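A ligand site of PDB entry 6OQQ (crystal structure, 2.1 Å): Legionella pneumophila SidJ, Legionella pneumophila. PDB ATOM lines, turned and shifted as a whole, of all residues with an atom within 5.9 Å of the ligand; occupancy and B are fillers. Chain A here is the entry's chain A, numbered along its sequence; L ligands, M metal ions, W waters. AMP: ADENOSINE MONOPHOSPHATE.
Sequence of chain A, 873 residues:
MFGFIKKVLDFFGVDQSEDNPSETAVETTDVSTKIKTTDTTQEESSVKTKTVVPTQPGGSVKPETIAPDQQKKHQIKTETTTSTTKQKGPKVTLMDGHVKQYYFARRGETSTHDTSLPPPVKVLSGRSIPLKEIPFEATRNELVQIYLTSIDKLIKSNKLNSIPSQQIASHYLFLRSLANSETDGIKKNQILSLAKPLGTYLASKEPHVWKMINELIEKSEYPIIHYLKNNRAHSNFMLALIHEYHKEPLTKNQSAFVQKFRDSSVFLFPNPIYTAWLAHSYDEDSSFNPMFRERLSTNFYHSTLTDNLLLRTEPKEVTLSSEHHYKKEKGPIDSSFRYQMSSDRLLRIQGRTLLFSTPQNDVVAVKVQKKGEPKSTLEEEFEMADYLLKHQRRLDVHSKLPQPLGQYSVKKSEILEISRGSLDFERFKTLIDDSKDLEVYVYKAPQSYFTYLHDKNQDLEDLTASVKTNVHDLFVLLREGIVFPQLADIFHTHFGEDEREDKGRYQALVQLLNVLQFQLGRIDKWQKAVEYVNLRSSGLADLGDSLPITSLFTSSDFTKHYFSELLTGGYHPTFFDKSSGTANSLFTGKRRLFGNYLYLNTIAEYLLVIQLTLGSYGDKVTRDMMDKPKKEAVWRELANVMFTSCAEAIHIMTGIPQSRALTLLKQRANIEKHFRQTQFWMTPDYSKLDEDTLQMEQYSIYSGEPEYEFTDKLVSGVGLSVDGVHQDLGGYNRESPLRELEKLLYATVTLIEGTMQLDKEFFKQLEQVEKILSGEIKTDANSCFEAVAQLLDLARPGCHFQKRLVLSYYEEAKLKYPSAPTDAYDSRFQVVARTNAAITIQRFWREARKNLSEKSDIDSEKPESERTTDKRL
A ring nitrogen (ND1) of His 492 sits at hydrogen-bond distance from the guanidinium group (NH2) of Arg 500 (3.4 Å). The guanidinium group (NH2) of Arg 500 lies within salt-bridge range of the side-chain carboxylate (OD2) of Asp 502, 2.7 Å away. The backbone NH (N) of His 492 lies within hydrogen-bond range of the backbone carbonyl oxygen (O) of Gly 504. The backbone carbonyl oxygen of His 492 sits at hydrogen-bond distance from the guanidinium group of Arg 522. The backbone NH (N) of Gly 504 is in hydrogen-bond range of the side-chain carboxylate (OD1) of Asp 502 (2.7 Å). The backbone carbonyl oxygen of Val 510 lies within hydrogen-bond range of the side-chain amide nitrogen of Asn 514. OH of Tyr 506 sits at hydrogen-bond distance from O of Gly 521. The side-chain amide nitrogen (ND2) of Asn 514 is in hydrogen-bond range of the side-chain amide oxygen (OE1) of Gln 507, at 2.6 Å.
Water W3 bridges OE1 of Gln 517 (2.9 Å) and O1P of the ligand (3.1 Å). Water W1 lies within hydrogen-bond range of a ring nitrogen (NE2) of His 492 (2.6 Å), the backbone carbonyl oxygen of Arg 734 (2.7 Å), the backbone NH of Arg 522 (3.4 Å) and an oxygen (O4') of the ligand (3.5 Å).
Merely in contact with the ligand: Tyr 506 (3.5 Å) and Val 510 (3.7 Å). Hydrophobic or aromatic side chains within 4 Å of the ligand: His 492, Tyr 506 and Val 510. 11 residues have an atom within 4 Å of the ligand: His 492, Arg 500, Asp 502, Arg 505, Tyr 506, Gln 507, Val 510, Gln 517, Gln 519, Gly 521 and Asn 733.
The side-chain amide oxygen of Asn 733 lies close to an oxygen (O2P) of the ligand, 2.9 Å away. The side-chain carboxylate (OD2) of Asp 502 is in hydrogen-bond range of a nitrogen (N6) of the ligand. The side-chain amide oxygen (OE1) of Gln 517 sits close to an oxygen (O2') of the ligand, 3.4 Å away. N of Gln 507 is in hydrogen-bond range of N1 of the ligand. An oxygen (O1P) of the ligand lies within salt-bridge range of the guanidinium group (NH2) of Arg 500 (2.8 Å). An oxygen (O2') of the ligand lies within hydrogen-bond range of the backbone carbonyl oxygen (O) of Gln 519. The backbone NH (N) of Gly 521 sits at hydrogen-bond distance from a nitrogen (N3) of the ligand (3.0 Å). An oxygen (O4') of the ligand lies within hydrogen-bond range of a ring nitrogen (NE2) of His 492, 3.0 Å away. The backbone carbonyl oxygen (O) of Arg 505 is in hydrogen-bond range of a nitrogen (N6) of the ligand.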
ATOM      1  N   HIS A 492       8.668 -13.573  11.574  1.00  0.00           N
ATOM      2  CA  HIS A 492       8.884 -14.435  12.724  1.00  0.00           C
ATOM      3  C   HIS A 492       9.181 -13.620  13.966  1.00  0.00           C
ATOM      4  O   HIS A 492       8.758 -13.982  15.076  1.00  0.00           O
ATOM      5  CB  HIS A 492      10.026 -15.423  12.466  1.00  0.00           C
ATOM      6  CG  HIS A 492      10.548 -16.070  13.708  1.00  0.00           C
ATOM      7  ND1 HIS A 492      11.859 -15.946  14.105  1.00  0.00           N
ATOM      8  CD2 HIS A 492       9.923 -16.821  14.647  1.00  0.00           C
ATOM      9  CE1 HIS A 492      12.029 -16.609  15.236  1.00  0.00           C
ATOM     10  NE2 HIS A 492      10.874 -17.146  15.584  1.00  0.00           N
ATOM     11  N   THR A 493       9.909 -12.516  13.808  1.00  0.00           N
ATOM     12  CA  THR A 493      10.241 -11.665  14.934  1.00  0.00           C
ATOM     13  C   THR A 493      10.618 -10.289  14.407  1.00  0.00           C
ATOM     14  O   THR A 493      10.931 -10.121  13.226  1.00  0.00           O
ATOM     15  CB  THR A 493      11.395 -12.254  15.764  1.00  0.00           C
ATOM     16  OG1 THR A 493      11.407 -11.660  17.066  1.00  0.00           O
ATOM     17  CG2 THR A 493      12.745 -11.989  15.080  1.00  0.00           C
ATOM     18  N   ARG A 500      19.420  -9.749  11.791  1.00  0.00           N
ATOM     19  CA  ARG A 500      19.113 -11.155  11.551  1.00  0.00           C
ATOM     20  C   ARG A 500      19.384 -11.496  10.094  1.00  0.00           C
ATOM     21  O   ARG A 500      19.035 -10.723   9.184  1.00  0.00           O
ATOM     22  CB  ARG A 500      17.656 -11.474  11.887  1.00  0.00           C
ATOM     23  CG  ARG A 500      17.348 -11.607  13.370  1.00  0.00           C
ATOM     24  CD  ARG A 500      15.871 -11.941  13.598  1.00  0.00           C
ATOM     25  NE  ARG A 500      15.551 -13.313  13.210  1.00  0.00           N
ATOM     26  CZ  ARG A 500      15.538 -14.352  14.039  1.00  0.00           C
ATOM     27  NH1 ARG A 500      15.818 -14.193  15.323  1.00  0.00           N
ATOM     28  NH2 ARG A 500      15.225 -15.556  13.576  1.00  0.00           N
ATOM     29  N   ASP A 502      17.811 -13.670   8.470  1.00  0.00           N
ATOM     30  CA  ASP A 502      16.493 -13.805   7.861  1.00  0.00           C
ATOM     31  C   ASP A 502      15.722 -12.489   7.802  1.00  0.00           C
ATOM     32  O   ASP A 502      14.630 -12.464   7.227  1.00  0.00           O
ATOM     33  CB  ASP A 502      15.676 -14.848   8.614  1.00  0.00           C
ATOM     34  CG  ASP A 502      15.411 -14.463  10.066  1.00  0.00           C
ATOM     35  OD1 ASP A 502      15.567 -13.270  10.406  1.00  0.00           O
ATOM     36  OD2 ASP A 502      15.053 -15.349  10.859  1.00  0.00           O
ATOM     37  N   GLY A 504      13.974 -11.170   9.886  1.00  0.00           N
ATOM     38  CA  GLY A 504      12.680 -11.340  10.515  1.00  0.00           C
ATOM     39  C   GLY A 504      11.608 -11.907   9.619  1.00  0.00           C
ATOM     40  O   GLY A 504      10.561 -12.338  10.130  1.00  0.00           O
ATOM     41  N   ARG A 505      11.840 -11.948   8.307  1.00  0.00           N
ATOM     42  CA  ARG A 505      10.849 -12.476   7.372  1.00  0.00           C
ATOM     43  C   ARG A 505      10.629 -13.959   7.649  1.00  0.00           C
ATOM     44  O   ARG A 505      11.588 -14.718   7.791  1.00  0.00           O
ATOM     45  CB  ARG A 505      11.319 -12.264   5.945  1.00  0.00           C
ATOM     46  CG  ARG A 505      10.295 -12.585   4.852  1.00  0.00           C
ATOM     47  CD  ARG A 505      10.949 -12.478   3.467  1.00  0.00           C
ATOM     48  NE  ARG A 505       9.983 -12.434   2.374  1.00  0.00           N
ATOM     49  CZ  ARG A 505       9.606 -13.494   1.644  1.00  0.00           C
ATOM     50  NH1 ARG A 505      10.090 -14.698   1.897  1.00  0.00           N
ATOM     51  NH2 ARG A 505       8.725 -13.330   0.663  1.00  0.00           N
ATOM     52  N   TYR A 506       9.371 -14.365   7.715  1.00  0.00           N
ATOM     53  CA  TYR A 506       9.061 -15.760   8.013  1.00  0.00           C
ATOM     54  C   TYR A 506       9.554 -16.652   6.869  1.00  0.00           C
ATOM     55  O   TYR A 506       9.449 -16.307   5.702  1.00  0.00           O
ATOM     56  CB  TYR A 506       7.561 -15.931   8.210  1.00  0.00           C
ATOM     57  CG  TYR A 506       7.184 -17.107   9.067  1.00  0.00           C
ATOM     58  CD1 TYR A 506       7.221 -17.025  10.456  1.00  0.00           C
ATOM     59  CD2 TYR A 506       6.773 -18.302   8.504  1.00  0.00           C
ATOM     60  CE1 TYR A 506       6.875 -18.091  11.254  1.00  0.00           C
ATOM     61  CE2 TYR A 506       6.410 -19.383   9.300  1.00  0.00           C
ATOM     62  CZ  TYR A 506       6.464 -19.274  10.669  1.00  0.00           C
ATOM     63  OH  TYR A 506       6.099 -20.344  11.443  1.00  0.00           O
ATOM     64  N   GLN A 507      10.095 -17.809   7.236  1.00  0.00           N
ATOM     65  CA  GLN A 507      10.522 -18.820   6.278  1.00  0.00           C
ATOM     66  C   GLN A 507       9.629 -20.045   6.455  1.00  0.00           C
ATOM     67  O   GLN A 507       9.714 -20.752   7.467  1.00  0.00           O
ATOM     68  CB  GLN A 507      12.001 -19.159   6.464  1.00  0.00           C
ATOM     69  CG  GLN A 507      12.916 -17.988   6.093  1.00  0.00           C
ATOM     70  CD  GLN A 507      14.386 -18.266   6.351  1.00  0.00           C
ATOM     71  OE1 GLN A 507      14.750 -19.308   6.904  1.00  0.00           O
ATOM     72  NE2 GLN A 507      15.240 -17.326   5.952  1.00  0.00           N
ATOM     73  N   ALA A 508       8.775 -20.301   5.451  1.00  0.00           N
ATOM     74  CA  ALA A 508       7.772 -21.351   5.563  1.00  0.00           C
ATOM     75  C   ALA A 508       8.392 -22.736   5.713  1.00  0.00           C
ATOM     76  O   ALA A 508       7.754 -23.633   6.252  1.00  0.00           O
ATOM     77  CB  ALA A 508       6.844 -21.325   4.357  1.00  0.00           C
ATOM     78  N   VAL A 510      11.592 -23.310   7.231  1.00  0.00           N
ATOM     79  CA  VAL A 510      12.811 -22.833   7.891  1.00  0.00           C
ATOM     80  C   VAL A 510      13.801 -23.965   8.139  1.00  0.00           C
ATOM     81  O   VAL A 510      15.020 -23.754   8.062  1.00  0.00           O
ATOM     82  CB  VAL A 510      12.450 -22.107   9.196  1.00  0.00           C
ATOM     83  CG1 VAL A 510      11.870 -23.075  10.228  1.00  0.00           C
ATOM     84  CG2 VAL A 510      13.668 -21.381   9.762  1.00  0.00           C
ATOM     85  N   GLN A 511      13.309 -25.171   8.441  1.00  0.00           N
ATOM     86  CA  GLN A 511      14.220 -26.276   8.743  1.00  0.00           C
ATOM     87  C   GLN A 511      15.158 -26.569   7.573  1.00  0.00           C
ATOM     88  O   GLN A 511      16.286 -27.034   7.784  1.00  0.00           O
ATOM     89  CB  GLN A 511      13.464 -27.552   9.104  1.00  0.00           C
ATOM     90  CG  GLN A 511      12.546 -27.442  10.290  1.00  0.00           C
ATOM     91  CD  GLN A 511      11.102 -27.181   9.884  1.00  0.00           C
ATOM     92  OE1 GLN A 511      10.841 -26.378   8.980  1.00  0.00           O
ATOM     93  NE2 GLN A 511      10.174 -27.856  10.546  1.00  0.00           N
ATOM     94  N   ASN A 514      18.083 -23.353   6.984  1.00  0.00           N
ATOM     95  CA  ASN A 514      18.983 -22.950   8.056  1.00  0.00           C
ATOM     96  C   ASN A 514      19.506 -24.207   8.735  1.00  0.00           C
ATOM     97  O   ASN A 514      18.924 -25.283   8.621  1.00  0.00           O
ATOM     98  CB  ASN A 514      18.272 -22.059   9.094  1.00  0.00           C
ATOM     99  CG  ASN A 514      17.651 -20.830   8.479  1.00  0.00           C
ATOM    100  OD1 ASN A 514      18.245 -19.751   8.489  1.00  0.00           O
ATOM    101  ND2 ASN A 514      16.446 -20.977   7.941  1.00  0.00           N
ATOM    102  N   GLN A 517      17.485 -25.822  12.815  1.00  0.00           N
ATOM    103  CA  GLN A 517      16.191 -25.242  13.112  1.00  0.00           C
ATOM    104  C   GLN A 517      15.149 -26.321  12.856  1.00  0.00           C
ATOM    105  O   GLN A 517      15.009 -26.791  11.720  1.00  0.00           O
ATOM    106  CB  GLN A 517      15.921 -24.005  12.251  1.00  0.00           C
ATOM    107  CG  GLN A 517      16.984 -22.920  12.379  1.00  0.00           C
ATOM    108  CD  GLN A 517      17.137 -22.414  13.795  1.00  0.00           C
ATOM    109  OE1 GLN A 517      16.248 -21.758  14.341  1.00  0.00           O
ATOM    110  NE2 GLN A 517      18.271 -22.730  14.412  1.00  0.00           N
ATOM    111  N   PHE A 518      14.443 -26.729  13.905  1.00  0.00           N
ATOM    112  CA  PHE A 518      13.664 -27.963  13.881  1.00  0.00           C
ATOM    113  C   PHE A 518      12.174 -27.747  13.683  1.00  0.00           C
ATOM    114  O   PHE A 518      11.458 -28.713  13.389  1.00  0.00           O
ATOM    115  CB  PHE A 518      13.886 -28.750  15.171  1.00  0.00           C
ATOM    116  CG  PHE A 518      15.333 -29.000  15.490  1.00  0.00           C
ATOM    117  CD1 PHE A 518      16.047 -29.967  14.803  1.00  0.00           C
ATOM    118  CD2 PHE A 518      15.971 -28.268  16.468  1.00  0.00           C
ATOM    119  CE1 PHE A 518      17.383 -30.197  15.088  1.00  0.00           C
ATOM    120  CE2 PHE A 518      17.306 -28.491  16.765  1.00  0.00           C
ATOM    121  CZ  PHE A 518      18.012 -29.454  16.066  1.00  0.00           C
ATOM    122  N   GLN A 519      11.675 -26.518  13.847  1.00  0.00           N
ATOM    123  CA  GLN A 519      10.237 -26.287  13.834  1.00  0.00           C
ATOM    124  C   GLN A 519       9.957 -24.880  13.318  1.00  0.00           C
ATOM    125  O   GLN A 519      10.770 -23.965  13.485  1.00  0.00           O
ATOM    126  CB  GLN A 519       9.624 -26.461  15.228  1.00  0.00           C
ATOM    127  CG  GLN A 519       9.736 -27.872  15.792  1.00  0.00           C
ATOM    128  CD  GLN A 519       9.001 -28.033  17.119  1.00  0.00           C
ATOM    129  OE1 GLN A 519       9.573 -27.827  18.184  1.00  0.00           O
ATOM    130  NE2 GLN A 519       7.728 -28.399  17.051  1.00  0.00           N
ATOM    131  N   LEU A 520       8.799 -24.726  12.683  1.00  0.00           N
ATOM    132  CA  LEU A 520       8.320 -23.407  12.300  1.00  0.00           C
ATOM    133  C   LEU A 520       8.096 -22.552  13.545  1.00  0.00           C
ATOM    134  O   LEU A 520       7.467 -22.995  14.504  1.00  0.00           O
ATOM    135  CB  LEU A 520       7.038 -23.525  11.496  1.00  0.00           C
ATOM    136  CG  LEU A 520       7.190 -23.576   9.977  1.00  0.00           C
ATOM    137  CD1 LEU A 520       8.159 -24.671   9.571  1.00  0.00           C
ATOM    138  CD2 LEU A 520       5.833 -23.797   9.326  1.00  0.00           C
ATOM    139  N   GLY A 521       8.605 -21.325  13.515  1.00  0.00           N
ATOM    140  CA  GLY A 521       8.649 -20.489  14.683  1.00  0.00           C
ATOM    141  C   GLY A 521       7.414 -19.623  14.851  1.00  0.00           C
ATOM    142  O   GLY A 521       6.494 -19.634  14.026  1.00  0.00           O
ATOM    143  N   ARG A 522       7.412 -18.866  15.949  1.00  0.00           N
ATOM    144  CA  ARG A 522       6.325 -17.938  16.229  1.00  0.00           C
ATOM    145  C   ARG A 522       6.044 -17.060  15.020  1.00  0.00           C
ATOM    146  O   ARG A 522       6.961 -16.584  14.354  1.00  0.00           O
ATOM    147  CB  ARG A 522       6.693 -17.076  17.450  1.00  0.00           C
ATOM    148  CG  ARG A 522       5.609 -16.108  17.912  1.00  0.00           C
ATOM    149  CD  ARG A 522       6.125 -15.208  19.049  1.00  0.00           C
ATOM    150  NE  ARG A 522       7.207 -14.344  18.587  1.00  0.00           N
ATOM    151  CZ  ARG A 522       7.083 -13.038  18.346  1.00  0.00           C
ATOM    152  NH1 ARG A 522       5.929 -12.409  18.560  1.00  0.00           N
ATOM    153  NH2 ARG A 522       8.142 -12.360  17.928  1.00  0.00           N
ATOM    154  N   ASN A 733      10.273 -16.848  21.470  1.00  0.00           N
ATOM    155  CA  ASN A 733      11.397 -17.763  21.269  1.00  0.00           C
ATOM    156  C   ASN A 733      10.960 -19.222  21.227  1.00  0.00           C
ATOM    157  O   ASN A 733      11.744 -20.126  21.519  1.00  0.00           O
ATOM    158  CB  ASN A 733      12.473 -17.556  22.348  1.00  0.00           C
ATOM    159  CG  ASN A 733      13.567 -16.617  21.914  1.00  0.00           C
ATOM    160  OD1 ASN A 733      14.039 -16.674  20.776  1.00  0.00           O
ATOM    161  ND2 ASN A 733      13.992 -15.733  22.813  1.00  0.00           N
ATOM    162  N   ARG A 734       9.716 -19.470  20.855  1.00  0.00           N
ATOM    163  CA  ARG A 734       9.188 -20.824  20.762  1.00  0.00           C
ATOM    164  C   ARG A 734       8.601 -21.044  19.374  1.00  0.00           C
ATOM    165  O   ARG A 734       8.606 -20.143  18.526  1.00  0.00           O
ATOM    166  CB  ARG A 734       8.158 -21.071  21.872  1.00  0.00           C
ATOM    167  CG  ARG A 734       8.789 -21.143  23.255  1.00  0.00           C
ATOM    168  CD  ARG A 734       7.771 -21.305  24.371  1.00  0.00           C
ATOM    169  NE  ARG A 734       8.415 -21.320  25.687  1.00  0.00           N
ATOM    170  CZ  ARG A 734       8.918 -22.413  26.271  1.00  0.00           C
ATOM    171  NH1 ARG A 734       8.845 -23.586  25.662  1.00  0.00           N
ATOM    172  NH2 ARG A 734       9.484 -22.322  27.466  1.00  0.00           N
ATOM    173  N   GLU A 735       8.103 -22.250  19.139  1.00  0.00           N
ATOM    174  CA  GLU A 735       7.620 -22.614  17.816  1.00  0.00           C
ATOM    175  C   GLU A 735       6.154 -22.238  17.653  1.00  0.00           C
ATOM    176  O   GLU A 735       5.459 -21.913  18.612  1.00  0.00           O
ATOM    177  CB  GLU A 735       7.823 -24.116  17.576  1.00  0.00           C
ATOM    178  CG  GLU A 735       6.828 -25.048  18.293  1.00  0.00           C
ATOM    179  CD  GLU A 735       7.196 -25.304  19.737  1.00  0.00           C
ATOM    180  OE1 GLU A 735       6.759 -26.346  20.285  1.00  0.00           O
ATOM    181  OE2 GLU A 735       7.909 -24.482  20.344  1.00  0.00           O
ATOM    182  N   SER A 736       5.694 -22.267  16.411  1.00  0.00           N
ATOM    183  CA  SER A 736       4.273 -22.124  16.142  1.00  0.00           C
ATOM    184  C   SER A 736       3.524 -23.338  16.680  1.00  0.00           C
ATOM    185  O   SER A 736       4.000 -24.468  16.559  1.00  0.00           O
ATOM    186  CB  SER A 736       4.016 -21.980  14.644  1.00  0.00           C
ATOM    187  OG  SER A 736       2.626 -22.065  14.367  1.00  0.00           O
HETATM  188  P   AMP L   1      14.899 -17.926  17.015  1.00  0.00           P
HETATM  189  O1P AMP L   1      15.381 -17.402  15.696  1.00  0.00           O
HETATM  190  O2P AMP L   1      14.353 -16.845  17.927  1.00  0.00           O
HETATM  191  O3P AMP L   1      15.843 -18.875  17.707  1.00  0.00           O
HETATM  192  O5' AMP L   1      13.620 -18.807  16.670  1.00  0.00           O
HETATM  193  C5' AMP L   1      13.278 -19.953  17.445  1.00  0.00           C
HETATM  194  C4' AMP L   1      12.177 -20.775  16.810  1.00  0.00           C
HETATM  195  O4' AMP L   1      11.666 -20.060  15.648  1.00  0.00           O
HETATM  196  C3' AMP L   1      12.598 -22.137  16.293  1.00  0.00           C
HETATM  197  O3' AMP L   1      11.474 -23.013  16.274  1.00  0.00           O
HETATM  198  C2' AMP L   1      13.032 -21.814  14.869  1.00  0.00           C
HETATM  199  O2' AMP L   1      13.055 -22.929  13.996  1.00  0.00           O
HETATM  200  C1' AMP L   1      11.983 -20.783  14.471  1.00  0.00           C
HETATM  201  N9  AMP L   1      12.421 -19.801  13.465  1.00  0.00           N
HETATM  202  C8  AMP L   1      13.557 -19.071  13.529  1.00  0.00           C
HETATM  203  N7  AMP L   1      13.633 -18.244  12.457  1.00  0.00           N
HETATM  204  C5  AMP L   1      12.541 -18.427  11.707  1.00  0.00           C
HETATM  205  C6  AMP L   1      11.996 -17.874  10.446  1.00  0.00           C
HETATM  206  N6  AMP L   1      12.675 -16.923   9.758  1.00  0.00           N
HETATM  207  N1  AMP L   1      10.812 -18.335   9.999  1.00  0.00           N
HETATM  208  C2  AMP L   1      10.127 -19.288  10.663  1.00  0.00           C
HETATM  209  N3  AMP L   1      10.562 -19.831  11.806  1.00  0.00           N
HETATM  210  C4  AMP L   1      11.733 -19.453  12.381  1.00  0.00           C
HETATM  211 MG    MG M   1      13.762 -13.103  18.836  1.00  0.00          MG
HETATM  212  O   HOH W   1      10.087 -17.974  17.914  1.00  0.00           O
HETATM  213  O   HOH W   2      16.817 -15.349  18.641  1.00  0.00           O
HETATM  214  O   HOH W   3      17.447 -19.097  14.052  1.00  0.00           O
